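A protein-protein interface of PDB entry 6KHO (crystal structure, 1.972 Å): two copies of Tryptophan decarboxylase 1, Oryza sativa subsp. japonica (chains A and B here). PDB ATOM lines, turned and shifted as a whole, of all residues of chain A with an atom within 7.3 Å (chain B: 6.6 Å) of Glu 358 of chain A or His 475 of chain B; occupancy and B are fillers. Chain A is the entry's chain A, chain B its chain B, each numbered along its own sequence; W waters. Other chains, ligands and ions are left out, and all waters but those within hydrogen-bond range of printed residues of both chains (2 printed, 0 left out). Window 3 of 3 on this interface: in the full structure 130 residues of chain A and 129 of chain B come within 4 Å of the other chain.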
ATOM      1  N   ASN A 356      22.915  26.158  -5.423  1.00  0.00           N
ATOM      2  CA  ASN A 356      23.852  26.661  -6.429  1.00  0.00           C
ATOM      3  C   ASN A 356      23.748  25.827  -7.700  1.00  0.00           C
ATOM      4  O   ASN A 356      24.738  25.265  -8.172  1.00  0.00           O
ATOM      5  CB  ASN A 356      25.281  26.681  -5.879  1.00  0.00           C
ATOM      6  CG  ASN A 356      26.211  27.593  -6.689  1.00  0.00           C
ATOM      7  OD1 ASN A 356      25.769  28.551  -7.337  1.00  0.00           O
ATOM      8  ND2 ASN A 356      27.505  27.291  -6.658  1.00  0.00           N
ATOM      9  N   PRO A 357      22.552  25.746  -8.294  1.00  0.00           N
ATOM     10  CA  PRO A 357      22.402  24.962  -9.525  1.00  0.00           C
ATOM     11  C   PRO A 357      23.154  25.615 -10.675  1.00  0.00           C
ATOM     12  O   PRO A 357      23.214  26.844 -10.786  1.00  0.00           O
ATOM     13  CB  PRO A 357      20.891  24.968  -9.766  1.00  0.00           C
ATOM     14  CG  PRO A 357      20.448  26.264  -9.205  1.00  0.00           C
ATOM     15  CD  PRO A 357      21.328  26.512  -7.987  1.00  0.00           C
ATOM     16  N   GLU A 358      23.727  24.767 -11.534  1.00  0.00           N
ATOM     17  CA  GLU A 358      24.620  25.244 -12.584  1.00  0.00           C
ATOM     18  C   GLU A 358      23.923  26.236 -13.511  1.00  0.00           C
ATOM     19  O   GLU A 358      24.518  27.247 -13.914  1.00  0.00           O
ATOM     20  CB  GLU A 358      25.150  24.049 -13.379  1.00  0.00           C
ATOM     21  CG  GLU A 358      26.086  24.405 -14.519  1.00  0.00           C
ATOM     22  CD  GLU A 358      27.424  24.929 -14.022  1.00  0.00           C
ATOM     23  OE1 GLU A 358      27.996  24.324 -13.082  1.00  0.00           O
ATOM     24  OE2 GLU A 358      27.889  25.961 -14.555  1.00  0.00           O
ATOM     25  N   TYR A 359      22.657  25.977 -13.842  1.00  0.00           N
ATOM     26  CA  TYR A 359      21.980  26.800 -14.846  1.00  0.00           C
ATOM     27  C   TYR A 359      21.731  28.234 -14.364  1.00  0.00           C
ATOM     28  O   TYR A 359      21.487  29.119 -15.195  1.00  0.00           O
ATOM     29  CB  TYR A 359      20.676  26.123 -15.293  1.00  0.00           C
ATOM     30  CG  TYR A 359      19.465  26.383 -14.415  1.00  0.00           C
ATOM     31  CD1 TYR A 359      19.326  25.764 -13.183  1.00  0.00           C
ATOM     32  CD2 TYR A 359      18.454  27.245 -14.829  1.00  0.00           C
ATOM     33  CE1 TYR A 359      18.225  26.006 -12.371  1.00  0.00           C
ATOM     34  CE2 TYR A 359      17.341  27.486 -14.033  1.00  0.00           C
ATOM     35  CZ  TYR A 359      17.232  26.872 -12.807  1.00  0.00           C
ATOM     36  OH  TYR A 359      16.127  27.116 -12.014  1.00  0.00           O
ATOM     37  N   LEU A 360      21.849  28.503 -13.065  1.00  0.00           N
ATOM     38  CA  LEU A 360      21.657  29.854 -12.543  1.00  0.00           C
ATOM     39  C   LEU A 360      22.962  30.585 -12.258  1.00  0.00           C
ATOM     40  O   LEU A 360      22.919  31.761 -11.870  1.00  0.00           O
ATOM     41  CB  LEU A 360      20.827  29.816 -11.262  1.00  0.00           C
ATOM     42  CG  LEU A 360      19.375  29.347 -11.397  1.00  0.00           C
ATOM     43  CD1 LEU A 360      18.681  29.397 -10.048  1.00  0.00           C
ATOM     44  CD2 LEU A 360      18.647  30.206 -12.385  1.00  0.00           C
ATOM     45  N   LYS A 361      24.112  29.929 -12.430  1.00  0.00           N
ATOM     46  CA  LYS A 361      25.384  30.551 -12.068  1.00  0.00           C
ATOM     47  C   LYS A 361      25.653  31.786 -12.917  1.00  0.00           C
ATOM     48  O   LYS A 361      25.313  31.828 -14.097  1.00  0.00           O
ATOM     49  CB  LYS A 361      26.525  29.544 -12.212  1.00  0.00           C
ATOM     50  CG  LYS A 361      26.516  28.505 -11.095  1.00  0.00           C
ATOM     51  CD  LYS A 361      27.613  27.471 -11.261  1.00  0.00           C
ATOM     52  CE  LYS A 361      27.603  26.477 -10.113  1.00  0.00           C
ATOM     53  NZ  LYS A 361      28.519  25.337 -10.398  1.00  0.00           N
ATOM     54  N   ASN A 362      26.258  32.802 -12.296  1.00  0.00           N
ATOM     55  CA  ASN A 362      26.573  34.043 -12.989  1.00  0.00           C
ATOM     56  C   ASN A 362      27.654  34.787 -12.214  1.00  0.00           C
ATOM     57  O   ASN A 362      27.869  34.555 -11.018  1.00  0.00           O
ATOM     58  CB  ASN A 362      25.329  34.926 -13.154  1.00  0.00           C
ATOM     59  CG  ASN A 362      24.757  35.364 -11.823  1.00  0.00           C
ATOM     60  OD1 ASN A 362      25.093  36.430 -11.308  1.00  0.00           O
ATOM     61  ND2 ASN A 362      23.922  34.513 -11.231  1.00  0.00           N
ATOM     62  N   PHE B 103      16.275  30.245 -19.344  1.00  0.00           N
ATOM     63  CA  PHE B 103      15.508  29.578 -18.276  1.00  0.00           C
ATOM     64  C   PHE B 103      14.273  28.933 -18.908  1.00  0.00           C
ATOM     65  O   PHE B 103      14.419  28.136 -19.841  1.00  0.00           O
ATOM     66  CB  PHE B 103      15.243  30.598 -17.168  1.00  0.00           C
ATOM     67  CG  PHE B 103      16.487  31.345 -16.739  1.00  0.00           C
ATOM     68  CD1 PHE B 103      17.602  30.644 -16.294  1.00  0.00           C
ATOM     69  CD2 PHE B 103      16.561  32.722 -16.827  1.00  0.00           C
ATOM     70  CE1 PHE B 103      18.768  31.314 -15.910  1.00  0.00           C
ATOM     71  CE2 PHE B 103      17.723  33.404 -16.455  1.00  0.00           C
ATOM     72  CZ  PHE B 103      18.833  32.692 -15.991  1.00  0.00           C
ATOM     73  N   SER B 215      17.363  21.206  -8.032  1.00  0.00           N
ATOM     74  CA  SER B 215      17.972  21.270  -6.704  1.00  0.00           C
ATOM     75  C   SER B 215      17.004  21.792  -5.650  1.00  0.00           C
ATOM     76  O   SER B 215      17.184  21.499  -4.462  1.00  0.00           O
ATOM     77  CB  SER B 215      19.230  22.144  -6.724  1.00  0.00           C
ATOM     78  OG  SER B 215      18.941  23.417  -7.282  1.00  0.00           O
ATOM     79  N   SER B 274      17.316  21.444 -16.770  1.00  0.00           N
ATOM     80  CA  SER B 274      18.558  21.567 -17.526  1.00  0.00           C
ATOM     81  C   SER B 274      18.361  21.203 -18.996  1.00  0.00           C
ATOM     82  O   SER B 274      18.655  22.004 -19.892  1.00  0.00           O
ATOM     83  CB  SER B 274      19.646  20.704 -16.881  1.00  0.00           C
ATOM     84  OG  SER B 274      20.817  20.725 -17.672  1.00  0.00           O
ATOM     85  N   ARG B 459      31.247  29.181 -23.762  1.00  0.00           N
ATOM     86  CA  ARG B 459      31.075  30.265 -22.801  1.00  0.00           C
ATOM     87  C   ARG B 459      31.300  31.614 -23.468  1.00  0.00           C
ATOM     88  O   ARG B 459      30.578  32.580 -23.193  1.00  0.00           O
ATOM     89  CB  ARG B 459      32.021  30.096 -21.605  1.00  0.00           C
ATOM     90  CG  ARG B 459      31.864  31.213 -20.568  1.00  0.00           C
ATOM     91  CD  ARG B 459      32.645  30.941 -19.262  1.00  0.00           C
ATOM     92  NE  ARG B 459      32.004  29.956 -18.381  1.00  0.00           N
ATOM     93  CZ  ARG B 459      30.965  30.214 -17.579  1.00  0.00           C
ATOM     94  NH1 ARG B 459      30.414  31.430 -17.545  1.00  0.00           N
ATOM     95  NH2 ARG B 459      30.465  29.252 -16.811  1.00  0.00           N
ATOM     96  N   MET B 462      28.269  32.564 -25.592  1.00  0.00           N
ATOM     97  CA  MET B 462      27.169  33.025 -24.750  1.00  0.00           C
ATOM     98  C   MET B 462      27.386  34.469 -24.308  1.00  0.00           C
ATOM     99  O   MET B 462      26.478  35.307 -24.397  1.00  0.00           O
ATOM    100  CB  MET B 462      27.035  32.096 -23.542  1.00  0.00           C
ATOM    101  CG  MET B 462      25.905  32.437 -22.570  1.00  0.00           C
ATOM    102  SD  MET B 462      25.967  31.389 -21.088  1.00  0.00           S
ATOM    103  CE  MET B 462      27.410  32.036 -20.237  1.00  0.00           C
ATOM    104  N   VAL B 473      21.008  34.450 -23.448  1.00  0.00           N
ATOM    105  CA  VAL B 473      21.217  33.015 -23.444  1.00  0.00           C
ATOM    106  C   VAL B 473      21.954  32.680 -22.158  1.00  0.00           C
ATOM    107  O   VAL B 473      22.785  33.465 -21.689  1.00  0.00           O
ATOM    108  CB  VAL B 473      22.010  32.567 -24.690  1.00  0.00           C
ATOM    109  CG1 VAL B 473      22.465  31.126 -24.569  1.00  0.00           C
ATOM    110  CG2 VAL B 473      21.142  32.746 -25.922  1.00  0.00           C
ATOM    111  N   ALA B 474      21.600  31.548 -21.560  1.00  0.00           N
ATOM    112  CA  ALA B 474      22.279  31.039 -20.384  1.00  0.00           C
ATOM    113  C   ALA B 474      22.547  29.557 -20.612  1.00  0.00           C
ATOM    114  O   ALA B 474      22.015  28.943 -21.544  1.00  0.00           O
ATOM    115  CB  ALA B 474      21.468  31.285 -19.100  1.00  0.00           C
ATOM    116  N   HIS B 475      23.381  28.991 -19.753  1.00  0.00           N
ATOM    117  CA  HIS B 475      24.027  27.715 -20.020  1.00  0.00           C
ATOM    118  C   HIS B 475      23.527  26.632 -19.071  1.00  0.00           C
ATOM    119  O   HIS B 475      22.739  26.874 -18.149  1.00  0.00           O
ATOM    120  CB  HIS B 475      25.545  27.863 -19.878  1.00  0.00           C
ATOM    121  CG  HIS B 475      25.993  27.904 -18.453  1.00  0.00           C
ATOM    122  ND1 HIS B 475      25.797  29.007 -17.647  1.00  0.00           N
ATOM    123  CD2 HIS B 475      26.579  26.964 -17.673  1.00  0.00           C
ATOM    124  CE1 HIS B 475      26.259  28.750 -16.436  1.00  0.00           C
ATOM    125  NE2 HIS B 475      26.736  27.517 -16.423  1.00  0.00           N
ATOM    126  N   THR B 476      23.990  25.413 -19.323  1.00  0.00           N
ATOM    127  CA  THR B 476      23.911  24.343 -18.344  1.00  0.00           C
ATOM    128  C   THR B 476      25.058  23.382 -18.628  1.00  0.00           C
ATOM    129  O   THR B 476      25.928  23.656 -19.459  1.00  0.00           O
ATOM    130  CB  THR B 476      22.544  23.649 -18.358  1.00  0.00           C
ATOM    131  OG1 THR B 476      22.457  22.776 -17.224  1.00  0.00           O
ATOM    132  CG2 THR B 476      22.328  22.860 -19.662  1.00  0.00           C
ATOM    133  N   VAL B 477      25.100  22.282 -17.887  1.00  0.00           N
ATOM    134  CA  VAL B 477      26.113  21.254 -18.090  1.00  0.00           C
ATOM    135  C   VAL B 477      25.388  19.934 -18.295  1.00  0.00           C
ATOM    136  O   VAL B 477      24.530  19.559 -17.488  1.00  0.00           O
ATOM    137  CB  VAL B 477      27.105  21.185 -16.912  1.00  0.00           C
ATOM    138  CG1 VAL B 477      27.967  19.925 -17.003  1.00  0.00           C
ATOM    139  CG2 VAL B 477      27.976  22.446 -16.894  1.00  0.00           C
ATOM    140  N   PHE B 482      29.882  21.872 -21.289  1.00  0.00           N
ATOM    141  CA  PHE B 482      29.233  23.175 -21.236  1.00  0.00           C
ATOM    142  C   PHE B 482      28.290  23.316 -22.437  1.00  0.00           C
ATOM    143  O   PHE B 482      28.705  23.152 -23.591  1.00  0.00           O
ATOM    144  CB  PHE B 482      30.308  24.263 -21.221  1.00  0.00           C
ATOM    145  CG  PHE B 482      29.803  25.655 -20.908  1.00  0.00           C
ATOM    146  CD1 PHE B 482      29.200  26.434 -21.895  1.00  0.00           C
ATOM    147  CD2 PHE B 482      29.989  26.209 -19.645  1.00  0.00           C
ATOM    148  CE1 PHE B 482      28.764  27.723 -21.619  1.00  0.00           C
ATOM    149  CE2 PHE B 482      29.555  27.503 -19.364  1.00  0.00           C
ATOM    150  CZ  PHE B 482      28.940  28.258 -20.349  1.00  0.00           C
ATOM    151  N   VAL B 483      27.016  23.601 -22.163  1.00  0.00           N
ATOM    152  CA  VAL B 483      25.942  23.529 -23.144  1.00  0.00           C
ATOM    153  C   VAL B 483      25.144  24.828 -23.089  1.00  0.00           C
ATOM    154  O   VAL B 483      24.934  25.380 -22.008  1.00  0.00           O
ATOM    155  CB  VAL B 483      25.045  22.306 -22.841  1.00  0.00           C
ATOM    156  CG1 VAL B 483      23.748  22.359 -23.609  1.00  0.00           C
ATOM    157  CG2 VAL B 483      25.803  21.013 -23.125  1.00  0.00           C
ATOM    158  N   LEU B 484      24.712  25.330 -24.250  1.00  0.00           N
ATOM    159  CA  LEU B 484      23.825  26.492 -24.299  1.00  0.00           C
ATOM    160  C   LEU B 484      22.377  26.016 -24.348  1.00  0.00           C
ATOM    161  O   LEU B 484      22.047  25.090 -25.096  1.00  0.00           O
ATOM    162  CB  LEU B 484      24.136  27.384 -25.508  1.00  0.00           C
ATOM    163  CG  LEU B 484      25.564  27.966 -25.574  1.00  0.00           C
ATOM    164  CD1 LEU B 484      25.677  29.070 -26.623  1.00  0.00           C
ATOM    165  CD2 LEU B 484      26.003  28.498 -24.230  1.00  0.00           C
ATOM    166  N   ARG B 485      21.527  26.604 -23.513  1.00  0.00           N
ATOM    167  CA  ARG B 485      20.094  26.360 -23.609  1.00  0.00           C
ATOM    168  C   ARG B 485      19.468  27.405 -24.521  1.00  0.00           C
ATOM    169  O   ARG B 485      19.927  28.550 -24.597  1.00  0.00           O
ATOM    170  CB  ARG B 485      19.421  26.400 -22.234  1.00  0.00           C
ATOM    171  CG  ARG B 485      19.811  25.256 -21.326  1.00  0.00           C
ATOM    172  CD  ARG B 485      19.327  25.470 -19.898  1.00  0.00           C
ATOM    173  NE  ARG B 485      17.949  25.005 -19.673  1.00  0.00           N
ATOM    174  CZ  ARG B 485      16.871  25.789 -19.714  1.00  0.00           C
ATOM    175  NH1 ARG B 485      16.984  27.081 -20.001  1.00  0.00           N
ATOM    176  NH2 ARG B 485      15.669  25.279 -19.477  1.00  0.00           N
HETATM  177  O   HOH W   1      20.556  28.444 -17.947  1.00  0.00           O
HETATM  178  O   HOH W   2      21.792  23.235 -14.083  1.00  0.00           O
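N of His 475 of chain B sits close to SD of Met 462 of chain B (3.8 Å). NZ of Lys 361 of chain A is in salt-bridge range of OE1 of Glu 358 of chain A. O of Leu 360 of chain A lies within hydrogen-bond range of ND2 of Asn 362 of chain A (3.0 Å). The backbone carbonyl oxygen (O) of Phe 103 of chain B sits at hydrogen-bond distance from the guanidinium group (NH1) of Arg 485 of chain B, at 2.8 Å.
Glu 358 of chain A touches just these residues of chain B: His 475 (2.7 Å) and Val 477 (3.6 Å). Of chain A, only Glu 358 (2.7 Å), Tyr 359 (3.4 Å) and Lys 361 (3.98 Å) come within 4 Å of His 475 of chain B. Of the printed residues of chain A, Phe 103 of chain B touches Tyr 359 and Leu 360. Printed residues of chain B within 4 Å of Leu 360 of chain A: Phe 103 (3.7 Å). Of the printed residues of chain B, Tyr 359 of chain A touches Phe 103 (3.6 Å) and His 475 (3.4 Å). Printed residues of chain B within 4 Å of Lys 361 of chain A: His 475. Thr 476 of chain B touches none of the printed residues of chain A.
Pro 357 of chain A touches Ser 215 of chain B. Val 477 of chain B touches Glu 358 of chain A (CG2 to CG, 3.6 Å). O of Tyr 359 of chain A touches CE1 of Phe 103 of chain B (3.6 Å). CA of Tyr 359 of chain A touches O of His 475 of chain B (3.4 Å). Phe 103 of chain B touches Leu 360 of chain A (CE1 to CD2, 3.7 Å). Lys 361 of chain A touches His 475 of chain B.
Water W1 lies within hydrogen-bond range of O of His 475 of chain B (2.7 Å) and O of Tyr 359 of chain A (3.0 Å). Water W2 bridges N of Tyr 359 of chain A (2.9 Å) and OG1 of Thr 476 of chain B (3.2 Å).
No position is printed for both chains.
Of the 14 printed residues of chain B, 4 touch a printed residue of chain A. Printed residues of chain B that touch a printed residue of chain A: Phe 103, Ser 215, His 475 and Val 477. Hydrophobic or aromatic side chains of chain B within 4 Å of the printed part of chain A: Phe 103, His 475 and Val 477. Hydrophobic or aromatic side chains of chain A within 4 Å of the printed part of chain B: Pro 357, Tyr 359 and Leu 360. Along chain A the printed residues that touch a printed residue of chain B span positions 357 to 361. Among the printed residues, no Asp or Glu carboxylate lies within 4 Å of a Lys or Arg side-chain nitrogen of the other chain.
OE2 of Glu 358 of chain A is in hydrogen-bond range of NE2 of His 475 of chain B, 2.7 Å away.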
